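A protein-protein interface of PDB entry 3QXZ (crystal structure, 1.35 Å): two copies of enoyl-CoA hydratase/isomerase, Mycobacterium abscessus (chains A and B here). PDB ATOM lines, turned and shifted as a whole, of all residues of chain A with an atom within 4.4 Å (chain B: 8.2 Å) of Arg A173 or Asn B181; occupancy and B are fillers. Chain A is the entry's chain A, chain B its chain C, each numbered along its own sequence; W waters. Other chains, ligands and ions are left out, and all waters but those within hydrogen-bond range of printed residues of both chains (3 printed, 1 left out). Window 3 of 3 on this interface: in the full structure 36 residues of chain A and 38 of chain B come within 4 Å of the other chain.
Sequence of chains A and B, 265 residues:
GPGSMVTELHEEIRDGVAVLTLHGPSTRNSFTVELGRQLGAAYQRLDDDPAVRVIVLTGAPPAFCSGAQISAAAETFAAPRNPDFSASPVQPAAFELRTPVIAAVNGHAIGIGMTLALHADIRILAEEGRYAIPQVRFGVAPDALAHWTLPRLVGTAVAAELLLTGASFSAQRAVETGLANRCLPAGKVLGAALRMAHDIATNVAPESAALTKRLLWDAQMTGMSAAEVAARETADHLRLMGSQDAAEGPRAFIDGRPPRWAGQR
Water W2 lies within hydrogen-bond range of O of Gly B178 (2.9 Å), N of Val A158 (2.9 Å) and N of Ala A157 (3.0 Å).
Water W1 bridges the side-chain carboxylate (OE2) of Glu A161 (2.9 Å) and the backbone carbonyl oxygen (O) of Asn B181 (3.5 Å).
Water W3 lies within hydrogen-bond range of the backbone carbonyl oxygen (O) of Ala B120 (3.0 Å), the guanidinium group (NH2) of Arg B123 (3.1 Å), the backbone carbonyl oxygen (O) of Asp B121 (3.2 Å) and the backbone NH (N) of Ala A157 (3.5 Å).
Among the printed residues, merely in contact across the chains: Ala A157 with Asp B121 (3.4 Å), Ala A157 with Arg B123 (3.4 Å), Ala A157 with Leu B153 (3.5 Å), Arg A173 with Asn B181 (3.7 Å), Val A158 with Asn B181 (3.9 Å), Ala A157 with Gly B178 (3.97 Å) and Glu A161 with Ile B122 (3.98 Å).
Printed residues of chain B within 4 Å of Arg A173: Asn B181.
Printed residues of chain A within 4 Å of Asn B181: Ala A157 (3.0 Å), Val A158 (3.9 Å), Glu A161 (2.8 Å) and Arg A173 (3.7 Å).
No residue of chain B comes within 4 Å of Ala A174.
Printed residues of chain A within 4 Å of Ile B122: Glu A161 (3.98 Å).
Of the printed residues of chain B, Glu A161 touches Ile B122 (3.98 Å) and Asn B181 (2.8 Å).
Of the printed residues of chain B, Val A158 touches Asn B181 (3.9 Å).
Printed residues of chain A within 4 Å of Arg B123: Ala A157.
The nearest printed residue of chain B that does not touch Arg A173 is Arg B182 (5.8 Å).
OE1 of Glu A161 sits at hydrogen-bond distance from ND2 of Asn B181 (2.8 Å).
The side-chain amide nitrogen (ND2) of Asn B181 sits at hydrogen-bond distance from the backbone carbonyl oxygen (O) of Ala A157, 3.0 Å away.
The side-chain hydroxyl (OG1) of Thr A177 lies within hydrogen-bond range of the backbone carbonyl oxygen (O) of Arg A173 (2.9 Å).
The backbone carbonyl oxygen (O) of Arg B123 is in hydrogen-bond range of the backbone NH (N) of Asn B181, 2.9 Å away.
The backbone NH of Ala B103 is in hydrogen-bond range of the backbone carbonyl oxygen of Ile B122 (2.8 Å).
N of Val B101 lies within hydrogen-bond range of OD2 of Asp B121 (2.8 Å).
The backbone NH (N) of Arg A173 lies within hydrogen-bond range of the side-chain hydroxyl (OG) of Ser A170 (3.0 Å).
The guanidinium group (NE) of Arg B123 lies within hydrogen-bond range of the backbone carbonyl oxygen (O) of Leu B179 (2.9 Å).
Positions printed for both chains: 171, 174, 175 and 176.
Of the 9 pairs that touch across the chains among the printed residues, none has its exchanged pair printed and touching as well.
Printed residues of chain A that touch a printed residue of chain B: Ala A157, Val A158, Glu A161 and Arg A173.
Hydrophobic or aromatic side chains of chain B that line the printed part of chain A: Ile B122 and Leu B153.
Among the printed residues, 9 pairs touch across the chains.
Among the printed residues, no Asp or Glu carboxylate lies within 4 Å of a Lys or Arg side-chain nitrogen of the other chain.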
ATOM      1  N   ALA A 157     -33.999 -14.112  12.601  1.00  0.00           N
ATOM      2  CA  ALA A 157     -32.690 -14.784  12.613  1.00  0.00           C
ATOM      3  C   ALA A 157     -31.803 -14.306  13.736  1.00  0.00           C
ATOM      4  O   ALA A 157     -31.203 -15.125  14.461  1.00  0.00           O
ATOM      5  CB  ALA A 157     -31.984 -14.621  11.258  1.00  0.00           C
ATOM      6  N   VAL A 158     -31.693 -12.993  13.889  1.00  0.00           N
ATOM      7  CA  VAL A 158     -30.937 -12.455  15.025  1.00  0.00           C
ATOM      8  C   VAL A 158     -31.602 -12.908  16.327  1.00  0.00           C
ATOM      9  O   VAL A 158     -30.916 -13.286  17.284  1.00  0.00           O
ATOM     10  CB  VAL A 158     -30.748 -10.926  14.944  1.00  0.00           C
ATOM     11  CG1 VAL A 158     -29.999 -10.416  16.175  1.00  0.00           C
ATOM     12  CG2 VAL A 158     -29.939 -10.552  13.676  1.00  0.00           C
ATOM     13  N   GLU A 161     -30.700 -16.585  16.965  1.00  0.00           N
ATOM     14  CA  GLU A 161     -29.312 -16.751  17.405  1.00  0.00           C
ATOM     15  C   GLU A 161     -29.189 -16.362  18.882  1.00  0.00           C
ATOM     16  O   GLU A 161     -28.613 -17.113  19.680  1.00  0.00           O
ATOM     17  CB  GLU A 161     -28.404 -15.854  16.577  1.00  0.00           C
ATOM     18  CG  GLU A 161     -26.947 -15.929  16.988  1.00  0.00           C
ATOM     19  CD  GLU A 161     -26.068 -14.940  16.245  1.00  0.00           C
ATOM     20  OE1 GLU A 161     -26.487 -14.329  15.254  1.00  0.00           O
ATOM     21  OE2 GLU A 161     -24.931 -14.747  16.710  1.00  0.00           O
ATOM     22  N   LEU A 162     -29.710 -15.204  19.287  1.00  0.00           N
ATOM     23  CA  LEU A 162     -29.530 -14.759  20.662  1.00  0.00           C
ATOM     24  C   LEU A 162     -30.270 -15.679  21.633  1.00  0.00           C
ATOM     25  O   LEU A 162     -29.732 -15.994  22.705  1.00  0.00           O
ATOM     26  CB  LEU A 162     -29.960 -13.296  20.818  1.00  0.00           C
ATOM     27  CG  LEU A 162     -29.171 -12.306  19.953  1.00  0.00           C
ATOM     28  CD1 LEU A 162     -29.582 -10.861  20.258  1.00  0.00           C
ATOM     29  CD2 LEU A 162     -27.652 -12.486  20.132  1.00  0.00           C
ATOM     30  N   SER A 170     -22.448  -7.280  21.489  1.00  0.00           N
ATOM     31  CA  SER A 170     -21.995  -5.944  21.846  1.00  0.00           C
ATOM     32  C   SER A 170     -23.099  -4.895  21.734  1.00  0.00           C
ATOM     33  O   SER A 170     -24.098  -5.073  21.023  1.00  0.00           O
ATOM     34  CB  SER A 170     -20.833  -5.529  20.947  1.00  0.00           C
ATOM     35  OG  SER A 170     -21.280  -5.314  19.614  1.00  0.00           O
ATOM     36  N   ALA A 171     -22.894  -3.766  22.400  1.00  0.00           N
ATOM     37  CA  ALA A 171     -23.768  -2.611  22.196  1.00  0.00           C
ATOM     38  C   ALA A 171     -23.861  -2.202  20.734  1.00  0.00           C
ATOM     39  O   ALA A 171     -24.941  -1.861  20.233  1.00  0.00           O
ATOM     40  CB  ALA A 171     -23.286  -1.421  23.025  1.00  0.00           C
ATOM     41  N   GLN A 172     -22.720  -2.231  20.041  1.00  0.00           N
ATOM     42  CA  GLN A 172     -22.703  -1.876  18.613  1.00  0.00           C
ATOM     43  C   GLN A 172     -23.574  -2.819  17.776  1.00  0.00           C
ATOM     44  O   GLN A 172     -24.325  -2.373  16.916  1.00  0.00           O
ATOM     45  CB  GLN A 172     -21.258  -1.787  18.062  1.00  0.00           C
ATOM     46  CG  GLN A 172     -21.175  -1.459  16.563  1.00  0.00           C
ATOM     47  CD  GLN A 172     -21.680  -0.062  16.192  1.00  0.00           C
ATOM     48  OE1 GLN A 172     -21.719   0.858  17.030  1.00  0.00           O
ATOM     49  NE2 GLN A 172     -22.056   0.108  14.920  1.00  0.00           N
ATOM     50  N   ARG A 173     -23.465  -4.125  18.019  1.00  0.00           N
ATOM     51  CA  ARG A 173     -24.320  -5.046  17.291  1.00  0.00           C
ATOM     52  C   ARG A 173     -25.797  -4.844  17.653  1.00  0.00           C
ATOM     53  O   ARG A 173     -26.656  -4.968  16.782  1.00  0.00           O
ATOM     54  CB  ARG A 173     -23.896  -6.498  17.474  1.00  0.00           C
ATOM     55  CG  ARG A 173     -24.551  -7.405  16.455  1.00  0.00           C
ATOM     56  CD  ARG A 173     -24.308  -8.859  16.751  1.00  0.00           C
ATOM     57  NE  ARG A 173     -25.039  -9.652  15.777  1.00  0.00           N
ATOM     58  CZ  ARG A 173     -25.277 -10.950  15.907  1.00  0.00           C
ATOM     59  NH1 ARG A 173     -24.854 -11.596  16.998  1.00  0.00           N
ATOM     60  NH2 ARG A 173     -25.952 -11.585  14.949  1.00  0.00           N
ATOM     61  N   ALA A 174     -26.080  -4.487  18.906  1.00  0.00           N
ATOM     62  CA  ALA A 174     -27.454  -4.182  19.304  1.00  0.00           C
ATOM     63  C   ALA A 174     -28.018  -3.014  18.499  1.00  0.00           C
ATOM     64  O   ALA A 174     -29.187  -3.040  18.084  1.00  0.00           O
ATOM     65  CB  ALA A 174     -27.514  -3.913  20.790  1.00  0.00           C
ATOM     66  N   VAL A 175     -27.210  -1.982  18.256  1.00  0.00           N
ATOM     67  CA  VAL A 175     -27.669  -0.868  17.436  1.00  0.00           C
ATOM     68  C   VAL A 175     -27.809  -1.284  15.978  1.00  0.00           C
ATOM     69  O   VAL A 175     -28.815  -0.973  15.342  1.00  0.00           O
ATOM     70  CB  VAL A 175     -26.714   0.349  17.546  1.00  0.00           C
ATOM     71  CG1 VAL A 175     -27.122   1.448  16.590  1.00  0.00           C
ATOM     72  CG2 VAL A 175     -26.668   0.863  18.971  1.00  0.00           C
ATOM     73  N   GLU A 176     -26.814  -2.000  15.448  1.00  0.00           N
ATOM     74  CA  GLU A 176     -26.832  -2.422  14.035  1.00  0.00           C
ATOM     75  C   GLU A 176     -28.065  -3.256  13.698  1.00  0.00           C
ATOM     76  O   GLU A 176     -28.618  -3.146  12.611  1.00  0.00           O
ATOM     77  CB  GLU A 176     -25.574  -3.226  13.683  1.00  0.00           C
ATOM     78  CG  GLU A 176     -24.305  -2.373  13.672  1.00  0.00           C
ATOM     79  CD  GLU A 176     -23.039  -3.196  13.674  1.00  0.00           C
ATOM     80  OE1 GLU A 176     -23.138  -4.441  13.803  1.00  0.00           O
ATOM     81  OE2 GLU A 176     -21.941  -2.586  13.557  1.00  0.00           O
ATOM     82  N   THR A 177     -28.507  -4.073  14.650  1.00  0.00           N
ATOM     83  CA  THR A 177     -29.612  -5.000  14.399  1.00  0.00           C
ATOM     84  C   THR A 177     -30.994  -4.454  14.747  1.00  0.00           C
ATOM     85  O   THR A 177     -31.984  -5.044  14.348  1.00  0.00           O
ATOM     86  CB  THR A 177     -29.410  -6.310  15.163  1.00  0.00           C
ATOM     87  OG1 THR A 177     -29.326  -6.042  16.565  1.00  0.00           O
ATOM     88  CG2 THR A 177     -28.152  -7.026  14.662  1.00  0.00           C
ATOM     89  N   VAL B 101     -31.738 -25.441  13.402  1.00  0.00           N
ATOM     90  CA  VAL B 101     -31.230 -25.635  12.030  1.00  0.00           C
ATOM     91  C   VAL B 101     -30.399 -24.425  11.664  1.00  0.00           C
ATOM     92  O   VAL B 101     -30.901 -23.275  11.699  1.00  0.00           O
ATOM     93  CB  VAL B 101     -32.388 -25.830  11.008  1.00  0.00           C
ATOM     94  CG1 VAL B 101     -31.835 -25.954   9.579  1.00  0.00           C
ATOM     95  CG2 VAL B 101     -33.212 -27.088  11.355  1.00  0.00           C
ATOM     96  N   ILE B 102     -29.149 -24.671  11.286  1.00  0.00           N
ATOM     97  CA  ILE B 102     -28.261 -23.618  10.795  1.00  0.00           C
ATOM     98  C   ILE B 102     -28.000 -23.871   9.312  1.00  0.00           C
ATOM     99  O   ILE B 102     -27.596 -24.984   8.930  1.00  0.00           O
ATOM    100  CB  ILE B 102     -26.931 -23.609  11.577  1.00  0.00           C
ATOM    101  CG1 ILE B 102     -27.167 -23.488  13.093  1.00  0.00           C
ATOM    102  CG2 ILE B 102     -25.943 -22.548  11.012  1.00  0.00           C
ATOM    103  CD1 ILE B 102     -25.897 -23.691  13.930  1.00  0.00           C
ATOM    104  N   ALA B 103     -28.227 -22.859   8.484  1.00  0.00           N
ATOM    105  CA  ALA B 103     -27.860 -22.981   7.065  1.00  0.00           C
ATOM    106  C   ALA B 103     -26.478 -22.391   6.858  1.00  0.00           C
ATOM    107  O   ALA B 103     -26.251 -21.184   7.058  1.00  0.00           O
ATOM    108  CB  ALA B 103     -28.891 -22.295   6.178  1.00  0.00           C
ATOM    109  N   ALA B 120     -34.201 -21.691   7.861  1.00  0.00           N
ATOM    110  CA  ALA B 120     -33.292 -22.012   8.977  1.00  0.00           C
ATOM    111  C   ALA B 120     -33.403 -20.946  10.076  1.00  0.00           C
ATOM    112  O   ALA B 120     -33.771 -19.781   9.830  1.00  0.00           O
ATOM    113  CB  ALA B 120     -31.845 -22.109   8.466  1.00  0.00           C
ATOM    114  N   ASP B 121     -33.018 -21.334  11.289  1.00  0.00           N
ATOM    115  CA  ASP B 121     -32.970 -20.388  12.411  1.00  0.00           C
ATOM    116  C   ASP B 121     -31.885 -19.356  12.216  1.00  0.00           C
ATOM    117  O   ASP B 121     -32.078 -18.167  12.503  1.00  0.00           O
ATOM    118  CB  ASP B 121     -32.733 -21.161  13.698  1.00  0.00           C
ATOM    119  CG  ASP B 121     -33.808 -22.183  13.943  1.00  0.00           C
ATOM    120  OD1 ASP B 121     -35.000 -21.812  13.904  1.00  0.00           O
ATOM    121  OD2 ASP B 121     -33.455 -23.371  14.164  1.00  0.00           O
ATOM    122  N   ILE B 122     -30.750 -19.819  11.699  1.00  0.00           N
ATOM    123  CA  ILE B 122     -29.515 -19.045  11.606  1.00  0.00           C
ATOM    124  C   ILE B 122     -28.919 -19.262  10.209  1.00  0.00           C
ATOM    125  O   ILE B 122     -28.942 -20.407   9.691  1.00  0.00           O
ATOM    126  CB  ILE B 122     -28.536 -19.512  12.710  1.00  0.00           C
ATOM    127  CG1 ILE B 122     -29.140 -19.193  14.100  1.00  0.00           C
ATOM    128  CG2 ILE B 122     -27.145 -18.889  12.529  1.00  0.00           C
ATOM    129  CD1 ILE B 122     -28.559 -20.024  15.269  1.00  0.00           C
ATOM    130  N   ARG B 123     -28.436 -18.190   9.584  1.00  0.00           N
ATOM    131  CA  ARG B 123     -27.752 -18.288   8.286  1.00  0.00           C
ATOM    132  C   ARG B 123     -26.373 -17.662   8.383  1.00  0.00           C
ATOM    133  O   ARG B 123     -26.217 -16.523   8.849  1.00  0.00           O
ATOM    134  CB  ARG B 123     -28.537 -17.555   7.178  1.00  0.00           C
ATOM    135  CG  ARG B 123     -29.566 -18.455   6.470  1.00  0.00           C
ATOM    136  CD  ARG B 123     -30.650 -17.670   5.648  1.00  0.00           C
ATOM    137  NE  ARG B 123     -31.378 -16.748   6.523  1.00  0.00           N
ATOM    138  CZ  ARG B 123     -32.214 -17.138   7.473  1.00  0.00           C
ATOM    139  NH1 ARG B 123     -32.614 -18.399   7.574  1.00  0.00           N
ATOM    140  NH2 ARG B 123     -32.700 -16.238   8.307  1.00  0.00           N
ATOM    141  N   ILE B 124     -25.380 -18.405   7.910  1.00  0.00           N
ATOM    142  CA  ILE B 124     -24.034 -17.889   7.723  1.00  0.00           C
ATOM    143  C   ILE B 124     -23.775 -17.938   6.219  1.00  0.00           C
ATOM    144  O   ILE B 124     -23.899 -19.007   5.599  1.00  0.00           O
ATOM    145  CB  ILE B 124     -23.012 -18.714   8.505  1.00  0.00           C
ATOM    146  CG1 ILE B 124     -23.358 -18.677  10.002  1.00  0.00           C
ATOM    147  CG2 ILE B 124     -21.594 -18.182   8.271  1.00  0.00           C
ATOM    148  CD1 ILE B 124     -22.422 -19.558  10.866  1.00  0.00           C
ATOM    149  N   LEU B 125     -23.488 -16.778   5.630  1.00  0.00           N
ATOM    150  CA  LEU B 125     -23.352 -16.670   4.154  1.00  0.00           C
ATOM    151  C   LEU B 125     -21.932 -16.432   3.704  1.00  0.00           C
ATOM    152  O   LEU B 125     -21.190 -15.666   4.341  1.00  0.00           O
ATOM    153  CB  LEU B 125     -24.263 -15.561   3.579  1.00  0.00           C
ATOM    154  CG  LEU B 125     -25.673 -15.988   3.124  1.00  0.00           C
ATOM    155  CD1 LEU B 125     -26.524 -16.596   4.227  1.00  0.00           C
ATOM    156  CD2 LEU B 125     -26.400 -14.766   2.559  1.00  0.00           C
ATOM    157  N   LEU B 153     -37.517 -10.963   8.514  1.00  0.00           N
ATOM    158  CA  LEU B 153     -36.064 -10.797   8.661  1.00  0.00           C
ATOM    159  C   LEU B 153     -35.612  -9.357   8.429  1.00  0.00           C
ATOM    160  O   LEU B 153     -34.856  -8.795   9.238  1.00  0.00           O
ATOM    161  CB  LEU B 153     -35.334 -11.708   7.666  1.00  0.00           C
ATOM    162  CG  LEU B 153     -35.509 -13.202   7.951  1.00  0.00           C
ATOM    163  CD1 LEU B 153     -35.065 -14.026   6.753  1.00  0.00           C
ATOM    164  CD2 LEU B 153     -34.747 -13.610   9.204  1.00  0.00           C
ATOM    165  N   ALA B 171     -23.949 -10.915   0.474  1.00  0.00           N
ATOM    166  CA  ALA B 171     -23.905 -11.407   1.852  1.00  0.00           C
ATOM    167  C   ALA B 171     -23.775 -10.251   2.852  1.00  0.00           C
ATOM    168  O   ALA B 171     -24.397 -10.275   3.924  1.00  0.00           O
ATOM    169  CB  ALA B 171     -22.750 -12.386   2.044  1.00  0.00           C
ATOM    170  N   ALA B 174     -27.059  -8.793   3.201  1.00  0.00           N
ATOM    171  CA  ALA B 174     -27.867  -9.747   3.966  1.00  0.00           C
ATOM    172  C   ALA B 174     -27.633  -9.596   5.467  1.00  0.00           C
ATOM    173  O   ALA B 174     -28.596  -9.652   6.257  1.00  0.00           O
ATOM    174  CB  ALA B 174     -27.576 -11.168   3.507  1.00  0.00           C
ATOM    175  N   VAL B 175     -26.397  -9.398   5.901  1.00  0.00           N
ATOM    176  CA  VAL B 175     -26.101  -9.235   7.321  1.00  0.00           C
ATOM    177  C   VAL B 175     -26.589  -7.868   7.796  1.00  0.00           C
ATOM    178  O   VAL B 175     -27.222  -7.767   8.851  1.00  0.00           O
ATOM    179  CB  VAL B 175     -24.590  -9.387   7.614  1.00  0.00           C
ATOM    180  CG1 VAL B 175     -24.264  -9.008   9.067  1.00  0.00           C
ATOM    181  CG2 VAL B 175     -24.149 -10.800   7.341  1.00  0.00           C
ATOM    182  N   GLU B 176     -26.346  -6.823   7.017  1.00  0.00           N
ATOM    183  CA  GLU B 176     -26.752  -5.461   7.393  1.00  0.00           C
ATOM    184  C   GLU B 176     -28.252  -5.325   7.564  1.00  0.00           C
ATOM    185  O   GLU B 176     -28.687  -4.520   8.409  1.00  0.00           O
ATOM    186  CB  GLU B 176     -26.296  -4.468   6.326  1.00  0.00           C
ATOM    187  CG  GLU B 176     -24.796  -4.219   6.323  1.00  0.00           C
ATOM    188  CD  GLU B 176     -24.306  -3.508   5.077  1.00  0.00           C
ATOM    189  OE1 GLU B 176     -25.105  -3.286   4.132  1.00  0.00           O
ATOM    190  OE2 GLU B 176     -23.081  -3.209   5.052  1.00  0.00           O
ATOM    191  N   GLY B 178     -30.496  -8.027   8.229  1.00  0.00           N
ATOM    192  CA  GLY B 178     -31.074  -8.968   9.158  1.00  0.00           C
ATOM    193  C   GLY B 178     -31.410 -10.323   8.539  1.00  0.00           C
ATOM    194  O   GLY B 178     -31.890 -11.217   9.222  1.00  0.00           O
ATOM    195  N   LEU B 179     -31.167 -10.491   7.245  1.00  0.00           N
ATOM    196  CA  LEU B 179     -31.440 -11.773   6.577  1.00  0.00           C
ATOM    197  C   LEU B 179     -30.474 -12.861   7.067  1.00  0.00           C
ATOM    198  O   LEU B 179     -30.867 -14.022   7.263  1.00  0.00           O
ATOM    199  CB  LEU B 179     -31.313 -11.626   5.068  1.00  0.00           C
ATOM    200  CG  LEU B 179     -31.683 -12.832   4.172  1.00  0.00           C
ATOM    201  CD1 LEU B 179     -32.192 -12.349   2.820  1.00  0.00           C
ATOM    202  CD2 LEU B 179     -30.530 -13.827   3.975  1.00  0.00           C
ATOM    203  N   ALA B 180     -29.211 -12.473   7.245  1.00  0.00           N
ATOM    204  CA  ALA B 180     -28.138 -13.379   7.642  1.00  0.00           C
ATOM    205  C   ALA B 180     -27.542 -12.950   8.952  1.00  0.00           C
ATOM    206  O   ALA B 180     -27.486 -11.764   9.270  1.00  0.00           O
ATOM    207  CB  ALA B 180     -27.047 -13.421   6.562  1.00  0.00           C
ATOM    208  N   ASN B 181     -27.058 -13.931   9.703  1.00  0.00           N
ATOM    209  CA  ASN B 181     -26.411 -13.685  10.996  1.00  0.00           C
ATOM    210  C   ASN B 181     -24.954 -13.283  10.874  1.00  0.00           C
ATOM    211  O   ASN B 181     -24.461 -12.500  11.708  1.00  0.00           O
ATOM    212  CB  ASN B 181     -26.510 -14.936  11.868  1.00  0.00           C
ATOM    213  CG  ASN B 181     -27.939 -15.337  12.103  1.00  0.00           C
ATOM    214  OD1 ASN B 181     -28.633 -15.836  11.203  1.00  0.00           O
ATOM    215  ND2 ASN B 181     -28.449 -15.004  13.311  1.00  0.00           N
ATOM    216  N   ARG B 182     -24.268 -13.805   9.852  1.00  0.00           N
ATOM    217  CA  ARG B 182     -22.846 -13.541   9.667  1.00  0.00           C
ATOM    218  C   ARG B 182     -22.502 -13.787   8.225  1.00  0.00           C
ATOM    219  O   ARG B 182     -23.177 -14.579   7.564  1.00  0.00           O
ATOM    220  CB  ARG B 182     -22.044 -14.464  10.562  1.00  0.00           C
ATOM    221  CG  ARG B 182     -20.597 -14.042  10.711  1.00  0.00           C
ATOM    222  CD  ARG B 182     -19.851 -14.934  11.689  1.00  0.00           C
ATOM    223  NE  ARG B 182     -18.467 -14.497  11.862  1.00  0.00           N
ATOM    224  CZ  ARG B 182     -17.542 -15.185  12.529  1.00  0.00           C
ATOM    225  NH1 ARG B 182     -17.847 -16.343  13.099  1.00  0.00           N
ATOM    226  NH2 ARG B 182     -16.305 -14.711  12.622  1.00  0.00           N
ATOM    227  N   CYS B 183     -21.474 -13.101   7.745  1.00  0.00           N
ATOM    228  CA  CYS B 183     -20.887 -13.437   6.469  1.00  0.00           C
ATOM    229  C   CYS B 183     -19.370 -13.590   6.603  1.00  0.00           C
ATOM    230  O   CYS B 183     -18.718 -12.893   7.391  1.00  0.00           O
ATOM    231  CB  CYS B 183     -21.288 -12.462   5.383  1.00  0.00           C
ATOM    232  SG  CYS B 183     -20.712 -10.806   5.592  1.00  0.00           S
ATOM    233  N   LEU B 184     -18.841 -14.543   5.852  1.00  0.00           N
ATOM    234  CA  LEU B 184     -17.455 -14.978   5.995  1.00  0.00           C
ATOM    235  C   LEU B 184     -16.977 -15.396   4.627  1.00  0.00           C
ATOM    236  O   LEU B 184     -17.790 -15.738   3.775  1.00  0.00           O
ATOM    237  CB  LEU B 184     -17.342 -16.182   6.947  1.00  0.00           C
ATOM    238  CG  LEU B 184     -17.552 -15.912   8.435  1.00  0.00           C
ATOM    239  CD1 LEU B 184     -17.750 -17.224   9.174  1.00  0.00           C
ATOM    240  CD2 LEU B 184     -16.367 -15.121   9.008  1.00  0.00           C
ATOM    241  N   MET B 196     -20.614 -23.191  15.833  1.00  0.00           N
ATOM    242  CA  MET B 196     -21.861 -22.770  16.466  1.00  0.00           C
ATOM    243  C   MET B 196     -22.740 -23.962  16.861  1.00  0.00           C
ATOM    244  O   MET B 196     -23.289 -24.002  17.972  1.00  0.00           O
ATOM    245  CB  MET B 196     -22.606 -21.820  15.535  1.00  0.00           C
ATOM    246  CG  MET B 196     -23.830 -21.204  16.163  1.00  0.00           C
ATOM    247  SD  MET B 196     -24.704 -20.089  15.060  1.00  0.00           S
ATOM    248  CE  MET B 196     -23.624 -18.677  15.076  1.00  0.00           C
HETATM  249  O   HOH W   1     -23.200 -14.148  14.477  1.00  0.00           O
HETATM  250  O   HOH W   2     -33.023 -11.347  11.840  1.00  0.00           O
HETATM  251  O   HOH W   3     -34.432 -16.988  10.729  1.00  0.00           O
